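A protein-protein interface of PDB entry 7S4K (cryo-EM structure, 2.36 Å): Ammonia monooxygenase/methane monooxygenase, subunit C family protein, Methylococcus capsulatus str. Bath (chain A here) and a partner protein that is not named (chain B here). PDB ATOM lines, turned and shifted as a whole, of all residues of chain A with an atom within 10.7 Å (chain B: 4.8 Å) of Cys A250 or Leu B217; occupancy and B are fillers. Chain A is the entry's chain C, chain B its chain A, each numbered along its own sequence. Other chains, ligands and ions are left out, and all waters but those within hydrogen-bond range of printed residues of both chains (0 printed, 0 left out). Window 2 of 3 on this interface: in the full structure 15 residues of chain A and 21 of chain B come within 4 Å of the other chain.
O of Leu B217 lies close to SG of Cys A250 (3.6 Å). OH of Tyr A238 lies close to OD2 of Asp B220, 2.3 Å away.
The backbone carbonyl oxygen (O) of Tyr A238 lies close to the side-chain amide oxygen (OE1) of Gln A242, at 3.2 Å. The backbone carbonyl oxygen (O) of Leu A249 sits close to the side-chain amide oxygen (OE1) of Gln A247, at 3.5 Å.
CD1 of Phe A237 touches CG1 of Ile B213 (3.8 Å). Leu B216 touches Phe A237. CD2 of Leu B216 touches CE1 of Tyr A238, at 3.9 Å. Leu A245 touches Leu B217. CD2 of Leu A249 touches CG2 of Ile B213, 3.5 Å away. Leu A249 touches Leu B217. Met B218 touches Cys A250.
Cys A250 touches just these residues of chain B: Leu B217 and Met B218. Leu B217 touches just these residues of chain A: Leu A245, Leu A249 and Cys A250. Ile B213 touches two residues of chain A. No residue of chain A comes within 4 Å of Pro B214. Leu B216 touches just these residues of chain A: Phe A237 and Tyr A238. Met B218 touches just one residue of chain A: Cys A250 (3.8 Å). Val B219 touches none of the printed residues of chain A. Asp B220 touches just one residue of chain A: Tyr A238. No residue of chain A comes within 4 Å of Ala B221. Of the printed residues of chain B, Phe A237 touches Ile B213 and Leu B216. Of the printed residues of chain B, Leu A245 touches Leu B217. Printed residues of chain B within 4 Å of Tyr A238: Leu B216 (3.9 Å) and Asp B220 (2.3 Å). Of the printed residues of chain B, Leu A249 touches Ile B213 (3.5 Å) and Leu B217 (3.9 Å). Arg B215 touches none of the printed residues of chain A. Ser A239 touches none of the printed residues of chain B. The nearest residue of chain A that does not touch Leu B217 is Ala A241 (4.9 Å).
Hydrophobic or aromatic side chains of chain A that line the printed part of chain B: Phe A237, Tyr A238, Leu A245 and Leu A249. Among the printed residues, 9 pairs touch across the chains.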
ATOM      1  N   THR A 234      -0.315  -3.826  -8.719  1.00  0.00           N
ATOM      2  CA  THR A 234      -1.651  -3.317  -9.015  1.00  0.00           C
ATOM      3  C   THR A 234      -1.592  -1.864  -9.476  1.00  0.00           C
ATOM      4  O   THR A 234      -2.386  -1.453 -10.334  1.00  0.00           O
ATOM      5  CB  THR A 234      -2.591  -3.480  -7.817  1.00  0.00           C
ATOM      6  OG1 THR A 234      -3.838  -2.835  -8.100  1.00  0.00           O
ATOM      7  CG2 THR A 234      -2.008  -2.879  -6.582  1.00  0.00           C
ATOM      8  N   GLN A 235      -0.635  -1.086  -8.964  1.00  0.00           N
ATOM      9  CA  GLN A 235      -0.443   0.263  -9.485  1.00  0.00           C
ATOM     10  C   GLN A 235      -0.007   0.242 -10.947  1.00  0.00           C
ATOM     11  O   GLN A 235      -0.494   1.041 -11.753  1.00  0.00           O
ATOM     12  CB  GLN A 235       0.574   1.006  -8.625  1.00  0.00           C
ATOM     13  CG  GLN A 235      -0.056   1.831  -7.529  1.00  0.00           C
ATOM     14  CD  GLN A 235       0.971   2.472  -6.634  1.00  0.00           C
ATOM     15  OE1 GLN A 235       2.166   2.238  -6.784  1.00  0.00           O
ATOM     16  NE2 GLN A 235       0.514   3.289  -5.697  1.00  0.00           N
ATOM     17  N   THR A 236       0.908  -0.661 -11.311  1.00  0.00           N
ATOM     18  CA  THR A 236       1.303  -0.763 -12.715  1.00  0.00           C
ATOM     19  C   THR A 236       0.167  -1.275 -13.586  1.00  0.00           C
ATOM     20  O   THR A 236       0.077  -0.903 -14.755  1.00  0.00           O
ATOM     21  CB  THR A 236       2.526  -1.665 -12.903  1.00  0.00           C
ATOM     22  OG1 THR A 236       2.126  -3.039 -12.890  1.00  0.00           O
ATOM     23  CG2 THR A 236       3.576  -1.415 -11.854  1.00  0.00           C
ATOM     24  N   PHE A 237      -0.698  -2.132 -13.047  1.00  0.00           N
ATOM     25  CA  PHE A 237      -1.861  -2.576 -13.807  1.00  0.00           C
ATOM     26  C   PHE A 237      -2.800  -1.413 -14.085  1.00  0.00           C
ATOM     27  O   PHE A 237      -3.327  -1.278 -15.194  1.00  0.00           O
ATOM     28  CB  PHE A 237      -2.589  -3.687 -13.055  1.00  0.00           C
ATOM     29  CG  PHE A 237      -1.865  -4.993 -13.066  1.00  0.00           C
ATOM     30  CD1 PHE A 237      -0.988  -5.304 -14.086  1.00  0.00           C
ATOM     31  CD2 PHE A 237      -2.056  -5.910 -12.051  1.00  0.00           C
ATOM     32  CE1 PHE A 237      -0.319  -6.505 -14.096  1.00  0.00           C
ATOM     33  CE2 PHE A 237      -1.390  -7.112 -12.056  1.00  0.00           C
ATOM     34  CZ  PHE A 237      -0.520  -7.409 -13.078  1.00  0.00           C
ATOM     35  N   TYR A 238      -3.024  -0.562 -13.082  1.00  0.00           N
ATOM     36  CA  TYR A 238      -3.850   0.619 -13.299  1.00  0.00           C
ATOM     37  C   TYR A 238      -3.201   1.573 -14.290  1.00  0.00           C
ATOM     38  O   TYR A 238      -3.886   2.179 -15.120  1.00  0.00           O
ATOM     39  CB  TYR A 238      -4.127   1.320 -11.972  1.00  0.00           C
ATOM     40  CG  TYR A 238      -5.164   0.609 -11.145  1.00  0.00           C
ATOM     41  CD1 TYR A 238      -6.266   0.021 -11.744  1.00  0.00           C
ATOM     42  CD2 TYR A 238      -5.040   0.516  -9.771  1.00  0.00           C
ATOM     43  CE1 TYR A 238      -7.216  -0.635 -10.998  1.00  0.00           C
ATOM     44  CE2 TYR A 238      -5.986  -0.138  -9.016  1.00  0.00           C
ATOM     45  CZ  TYR A 238      -7.071  -0.712  -9.633  1.00  0.00           C
ATOM     46  OH  TYR A 238      -8.014  -1.364  -8.880  1.00  0.00           O
ATOM     47  N   SER A 239      -1.878   1.723 -14.218  1.00  0.00           N
ATOM     48  CA  SER A 239      -1.173   2.542 -15.200  1.00  0.00           C
ATOM     49  C   SER A 239      -1.312   1.971 -16.605  1.00  0.00           C
ATOM     50  O   SER A 239      -1.488   2.726 -17.566  1.00  0.00           O
ATOM     51  CB  SER A 239       0.300   2.663 -14.817  1.00  0.00           C
ATOM     52  OG  SER A 239       1.119   2.759 -15.965  1.00  0.00           O
ATOM     53  N   PHE A 240      -1.231   0.648 -16.737  1.00  0.00           N
ATOM     54  CA  PHE A 240      -1.450  -0.010 -18.018  1.00  0.00           C
ATOM     55  C   PHE A 240      -2.854   0.256 -18.537  1.00  0.00           C
ATOM     56  O   PHE A 240      -3.042   0.555 -19.721  1.00  0.00           O
ATOM     57  CB  PHE A 240      -1.230  -1.513 -17.863  1.00  0.00           C
ATOM     58  CG  PHE A 240       0.041  -2.015 -18.470  1.00  0.00           C
ATOM     59  CD1 PHE A 240       0.211  -2.039 -19.840  1.00  0.00           C
ATOM     60  CD2 PHE A 240       1.064  -2.483 -17.666  1.00  0.00           C
ATOM     61  CE1 PHE A 240       1.378  -2.515 -20.396  1.00  0.00           C
ATOM     62  CE2 PHE A 240       2.231  -2.958 -18.217  1.00  0.00           C
ATOM     63  CZ  PHE A 240       2.388  -2.974 -19.582  1.00  0.00           C
ATOM     64  N   ALA A 241      -3.849   0.141 -17.666  1.00  0.00           N
ATOM     65  CA  ALA A 241      -5.255   0.307 -18.030  1.00  0.00           C
ATOM     66  C   ALA A 241      -5.726   1.736 -17.802  1.00  0.00           C
ATOM     67  O   ALA A 241      -6.748   1.975 -17.162  1.00  0.00           O
ATOM     68  CB  ALA A 241      -6.108  -0.681 -17.247  1.00  0.00           C
ATOM     69  N   GLN A 242      -4.988   2.713 -18.325  1.00  0.00           N
ATOM     70  CA  GLN A 242      -5.388   4.120 -18.209  1.00  0.00           C
ATOM     71  C   GLN A 242      -6.161   4.537 -19.455  1.00  0.00           C
ATOM     72  O   GLN A 242      -7.324   4.939 -19.372  1.00  0.00           O
ATOM     73  CB  GLN A 242      -4.161   5.008 -17.990  1.00  0.00           C
ATOM     74  CG  GLN A 242      -3.627   5.077 -16.555  1.00  0.00           C
ATOM     75  CD  GLN A 242      -4.659   5.522 -15.527  1.00  0.00           C
ATOM     76  OE1 GLN A 242      -5.680   4.868 -15.313  1.00  0.00           O
ATOM     77  NE2 GLN A 242      -4.387   6.649 -14.882  1.00  0.00           N
ATOM     78  N   GLY A 243      -5.518   4.445 -20.616  1.00  0.00           N
ATOM     79  CA  GLY A 243      -6.184   4.688 -21.878  1.00  0.00           C
ATOM     80  C   GLY A 243      -6.334   3.413 -22.680  1.00  0.00           C
ATOM     81  O   GLY A 243      -7.340   3.208 -23.363  1.00  0.00           O
ATOM     82  N   GLY A 244      -5.332   2.542 -22.587  1.00  0.00           N
ATOM     83  CA  GLY A 244      -5.339   1.288 -23.312  1.00  0.00           C
ATOM     84  C   GLY A 244      -5.992   0.167 -22.532  1.00  0.00           C
ATOM     85  O   GLY A 244      -5.712  -1.012 -22.765  1.00  0.00           O
ATOM     86  N   LEU A 245      -6.866   0.533 -21.594  1.00  0.00           N
ATOM     87  CA  LEU A 245      -7.596  -0.454 -20.814  1.00  0.00           C
ATOM     88  C   LEU A 245      -8.465  -1.341 -21.687  1.00  0.00           C
ATOM     89  O   LEU A 245      -8.529  -2.551 -21.450  1.00  0.00           O
ATOM     90  CB  LEU A 245      -8.457   0.251 -19.758  1.00  0.00           C
ATOM     91  CG  LEU A 245      -9.545  -0.470 -18.951  1.00  0.00           C
ATOM     92  CD1 LEU A 245      -9.802   0.303 -17.668  1.00  0.00           C
ATOM     93  CD2 LEU A 245     -10.858  -0.612 -19.717  1.00  0.00           C
ATOM     94  N   GLY A 246      -9.128  -0.767 -22.686  1.00  0.00           N
ATOM     95  CA  GLY A 246     -10.047  -1.514 -23.513  1.00  0.00           C
ATOM     96  C   GLY A 246     -10.059  -0.984 -24.930  1.00  0.00           C
ATOM     97  O   GLY A 246      -9.289  -0.095 -25.297  1.00  0.00           O
ATOM     98  N   GLN A 247     -10.971  -1.536 -25.719  1.00  0.00           N
ATOM     99  CA  GLN A 247     -11.927  -2.474 -25.156  1.00  0.00           C
ATOM    100  C   GLN A 247     -11.694  -3.901 -25.621  1.00  0.00           C
ATOM    101  O   GLN A 247     -10.958  -4.143 -26.579  1.00  0.00           O
ATOM    102  CB  GLN A 247     -13.355  -2.029 -25.471  1.00  0.00           C
ATOM    103  CG  GLN A 247     -13.663  -0.650 -24.915  1.00  0.00           C
ATOM    104  CD  GLN A 247     -13.664  -0.634 -23.395  1.00  0.00           C
ATOM    105  OE1 GLN A 247     -14.071  -1.602 -22.753  1.00  0.00           O
ATOM    106  NE2 GLN A 247     -13.195   0.464 -22.813  1.00  0.00           N
ATOM    107  N   SER A 248     -12.414  -4.807 -24.956  1.00  0.00           N
ATOM    108  CA  SER A 248     -12.106  -6.222 -24.775  1.00  0.00           C
ATOM    109  C   SER A 248     -12.354  -6.538 -23.310  1.00  0.00           C
ATOM    110  O   SER A 248     -13.345  -7.184 -22.953  1.00  0.00           O
ATOM    111  CB  SER A 248     -10.662  -6.573 -25.137  1.00  0.00           C
ATOM    112  OG  SER A 248     -10.265  -7.785 -24.520  1.00  0.00           O
ATOM    113  N   LEU A 249     -11.437  -6.085 -22.465  1.00  0.00           N
ATOM    114  CA  LEU A 249     -11.560  -6.229 -21.023  1.00  0.00           C
ATOM    115  C   LEU A 249     -12.800  -5.506 -20.515  1.00  0.00           C
ATOM    116  O   LEU A 249     -13.058  -4.358 -20.891  1.00  0.00           O
ATOM    117  CB  LEU A 249     -10.302  -5.675 -20.346  1.00  0.00           C
ATOM    118  CG  LEU A 249      -8.957  -6.418 -20.383  1.00  0.00           C
ATOM    119  CD1 LEU A 249      -8.646  -7.091 -21.714  1.00  0.00           C
ATOM    120  CD2 LEU A 249      -7.849  -5.446 -20.037  1.00  0.00           C
ATOM    121  N   CYS A 250     -13.563  -6.184 -19.657  1.00  0.00           N
ATOM    122  CA  CYS A 250     -14.765  -5.625 -19.032  1.00  0.00           C
ATOM    123  C   CYS A 250     -15.757  -5.103 -20.068  1.00  0.00           C
ATOM    124  O   CYS A 250     -16.285  -3.994 -19.957  1.00  0.00           O
ATOM    125  CB  CYS A 250     -14.405  -4.534 -18.024  1.00  0.00           C
ATOM    126  SG  CYS A 250     -14.341  -5.107 -16.313  1.00  0.00           S
ATOM    127  N   GLU A 251     -16.013  -5.918 -21.086  1.00  0.00           N
ATOM    128  CA  GLU A 251     -17.049  -5.611 -22.068  1.00  0.00           C
ATOM    129  C   GLU A 251     -17.437  -6.864 -22.847  1.00  0.00           C
ATOM    130  O   GLU A 251     -18.612  -7.225 -22.914  1.00  0.00           O
ATOM    131  CB  GLU A 251     -16.584  -4.505 -23.023  1.00  0.00           C
ATOM    132  CG  GLU A 251     -15.438  -4.888 -23.938  1.00  0.00           C
ATOM    133  CD  GLU A 251     -15.907  -5.480 -25.255  1.00  0.00           C
ATOM    134  OE1 GLU A 251     -17.128  -5.468 -25.513  1.00  0.00           O
ATOM    135  OE2 GLU A 251     -15.056  -5.957 -26.031  1.00  0.00           O
ATOM    136  N   ILE B 213      -5.260  -8.514 -15.412  1.00  0.00           N
ATOM    137  CA  ILE B 213      -5.931  -7.229 -15.613  1.00  0.00           C
ATOM    138  C   ILE B 213      -7.435  -7.408 -15.809  1.00  0.00           C
ATOM    139  O   ILE B 213      -8.212  -6.681 -15.173  1.00  0.00           O
ATOM    140  CB  ILE B 213      -5.307  -6.440 -16.776  1.00  0.00           C
ATOM    141  CG1 ILE B 213      -3.842  -6.125 -16.477  1.00  0.00           C
ATOM    142  CG2 ILE B 213      -6.066  -5.148 -16.996  1.00  0.00           C
ATOM    143  CD1 ILE B 213      -3.256  -5.044 -17.359  1.00  0.00           C
ATOM    144  N   PRO B 214      -7.907  -8.317 -16.673  1.00  0.00           N
ATOM    145  CA  PRO B 214      -9.363  -8.517 -16.751  1.00  0.00           C
ATOM    146  C   PRO B 214      -9.984  -8.947 -15.436  1.00  0.00           C
ATOM    147  O   PRO B 214     -11.076  -8.481 -15.097  1.00  0.00           O
ATOM    148  CB  PRO B 214      -9.513  -9.591 -17.838  1.00  0.00           C
ATOM    149  CG  PRO B 214      -8.183 -10.211 -17.956  1.00  0.00           C
ATOM    150  CD  PRO B 214      -7.210  -9.125 -17.686  1.00  0.00           C
ATOM    151  N   ARG B 215      -9.311  -9.806 -14.667  1.00  0.00           N
ATOM    152  CA  ARG B 215      -9.868 -10.231 -13.387  1.00  0.00           C
ATOM    153  C   ARG B 215      -9.861  -9.092 -12.376  1.00  0.00           C
ATOM    154  O   ARG B 215     -10.810  -8.940 -11.598  1.00  0.00           O
ATOM    155  CB  ARG B 215      -9.100 -11.437 -12.853  1.00  0.00           C
ATOM    156  CG  ARG B 215      -9.454 -12.732 -13.557  1.00  0.00           C
ATOM    157  CD  ARG B 215      -8.700 -13.910 -12.979  1.00  0.00           C
ATOM    158  NE  ARG B 215      -9.348 -14.455 -11.795  1.00  0.00           N
ATOM    159  CZ  ARG B 215     -10.216 -15.456 -11.813  1.00  0.00           C
ATOM    160  NH1 ARG B 215     -10.584 -16.029 -12.946  1.00  0.00           N
ATOM    161  NH2 ARG B 215     -10.727 -15.892 -10.667  1.00  0.00           N
ATOM    162  N   LEU B 216      -8.801  -8.279 -12.372  1.00  0.00           N
ATOM    163  CA  LEU B 216      -8.770  -7.109 -11.504  1.00  0.00           C
ATOM    164  C   LEU B 216      -9.910  -6.160 -11.835  1.00  0.00           C
ATOM    165  O   LEU B 216     -10.593  -5.658 -10.936  1.00  0.00           O
ATOM    166  CB  LEU B 216      -7.430  -6.390 -11.642  1.00  0.00           C
ATOM    167  CG  LEU B 216      -7.286  -5.047 -10.928  1.00  0.00           C
ATOM    168  CD1 LEU B 216      -7.245  -5.246  -9.426  1.00  0.00           C
ATOM    169  CD2 LEU B 216      -6.048  -4.316 -11.406  1.00  0.00           C
ATOM    170  N   LEU B 217     -10.139  -5.918 -13.125  1.00  0.00           N
ATOM    171  CA  LEU B 217     -11.217  -5.023 -13.529  1.00  0.00           C
ATOM    172  C   LEU B 217     -12.581  -5.611 -13.191  1.00  0.00           C
ATOM    173  O   LEU B 217     -13.497  -4.876 -12.813  1.00  0.00           O
ATOM    174  CB  LEU B 217     -11.108  -4.720 -15.021  1.00  0.00           C
ATOM    175  CG  LEU B 217      -9.875  -3.918 -15.438  1.00  0.00           C
ATOM    176  CD1 LEU B 217      -9.750  -3.875 -16.950  1.00  0.00           C
ATOM    177  CD2 LEU B 217      -9.915  -2.519 -14.857  1.00  0.00           C
ATOM    178  N   MET B 218     -12.741  -6.928 -13.330  1.00  0.00           N
ATOM    179  CA  MET B 218     -14.016  -7.551 -12.992  1.00  0.00           C
ATOM    180  C   MET B 218     -14.291  -7.479 -11.495  1.00  0.00           C
ATOM    181  O   MET B 218     -15.434  -7.264 -11.080  1.00  0.00           O
ATOM    182  CB  MET B 218     -14.040  -8.999 -13.474  1.00  0.00           C
ATOM    183  CG  MET B 218     -14.214  -9.146 -14.974  1.00  0.00           C
ATOM    184  SD  MET B 218     -15.934  -9.057 -15.499  1.00  0.00           S
ATOM    185  CE  MET B 218     -16.649 -10.400 -14.558  1.00  0.00           C
ATOM    186  N   VAL B 219     -13.261  -7.668 -10.669  1.00  0.00           N
ATOM    187  CA  VAL B 219     -13.452  -7.558  -9.227  1.00  0.00           C
ATOM    188  C   VAL B 219     -13.737  -6.113  -8.836  1.00  0.00           C
ATOM    189  O   VAL B 219     -14.579  -5.843  -7.973  1.00  0.00           O
ATOM    190  CB  VAL B 219     -12.232  -8.121  -8.476  1.00  0.00           C
ATOM    191  CG1 VAL B 219     -12.354  -7.853  -6.989  1.00  0.00           C
ATOM    192  CG2 VAL B 219     -12.094  -9.607  -8.731  1.00  0.00           C
ATOM    193  N   ASP B 220     -13.049  -5.161  -9.470  1.00  0.00           N
ATOM    194  CA  ASP B 220     -13.242  -3.748  -9.149  1.00  0.00           C
ATOM    195  C   ASP B 220     -14.631  -3.275  -9.565  1.00  0.00           C
ATOM    196  O   ASP B 220     -15.428  -2.837  -8.730  1.00  0.00           O
ATOM    197  CB  ASP B 220     -12.160  -2.908  -9.835  1.00  0.00           C
ATOM    198  CG  ASP B 220     -10.819  -3.012  -9.149  1.00  0.00           C
ATOM    199  OD1 ASP B 220     -10.737  -3.683  -8.100  1.00  0.00           O
ATOM    200  OD2 ASP B 220      -9.843  -2.429  -9.664  1.00  0.00           O
ATOM    201  N   ALA B 221     -14.933  -3.363 -10.857  1.00  0.00           N
ATOM    202  CA  ALA B 221     -16.198  -2.890 -11.394  1.00  0.00           C
ATOM    203  C   ALA B 221     -17.330  -3.812 -10.975  1.00  0.00           C
ATOM    204  O   ALA B 221     -17.607  -4.814 -11.641  1.00  0.00           O
ATOM    205  CB  ALA B 221     -16.130  -2.792 -12.919  1.00  0.00           C
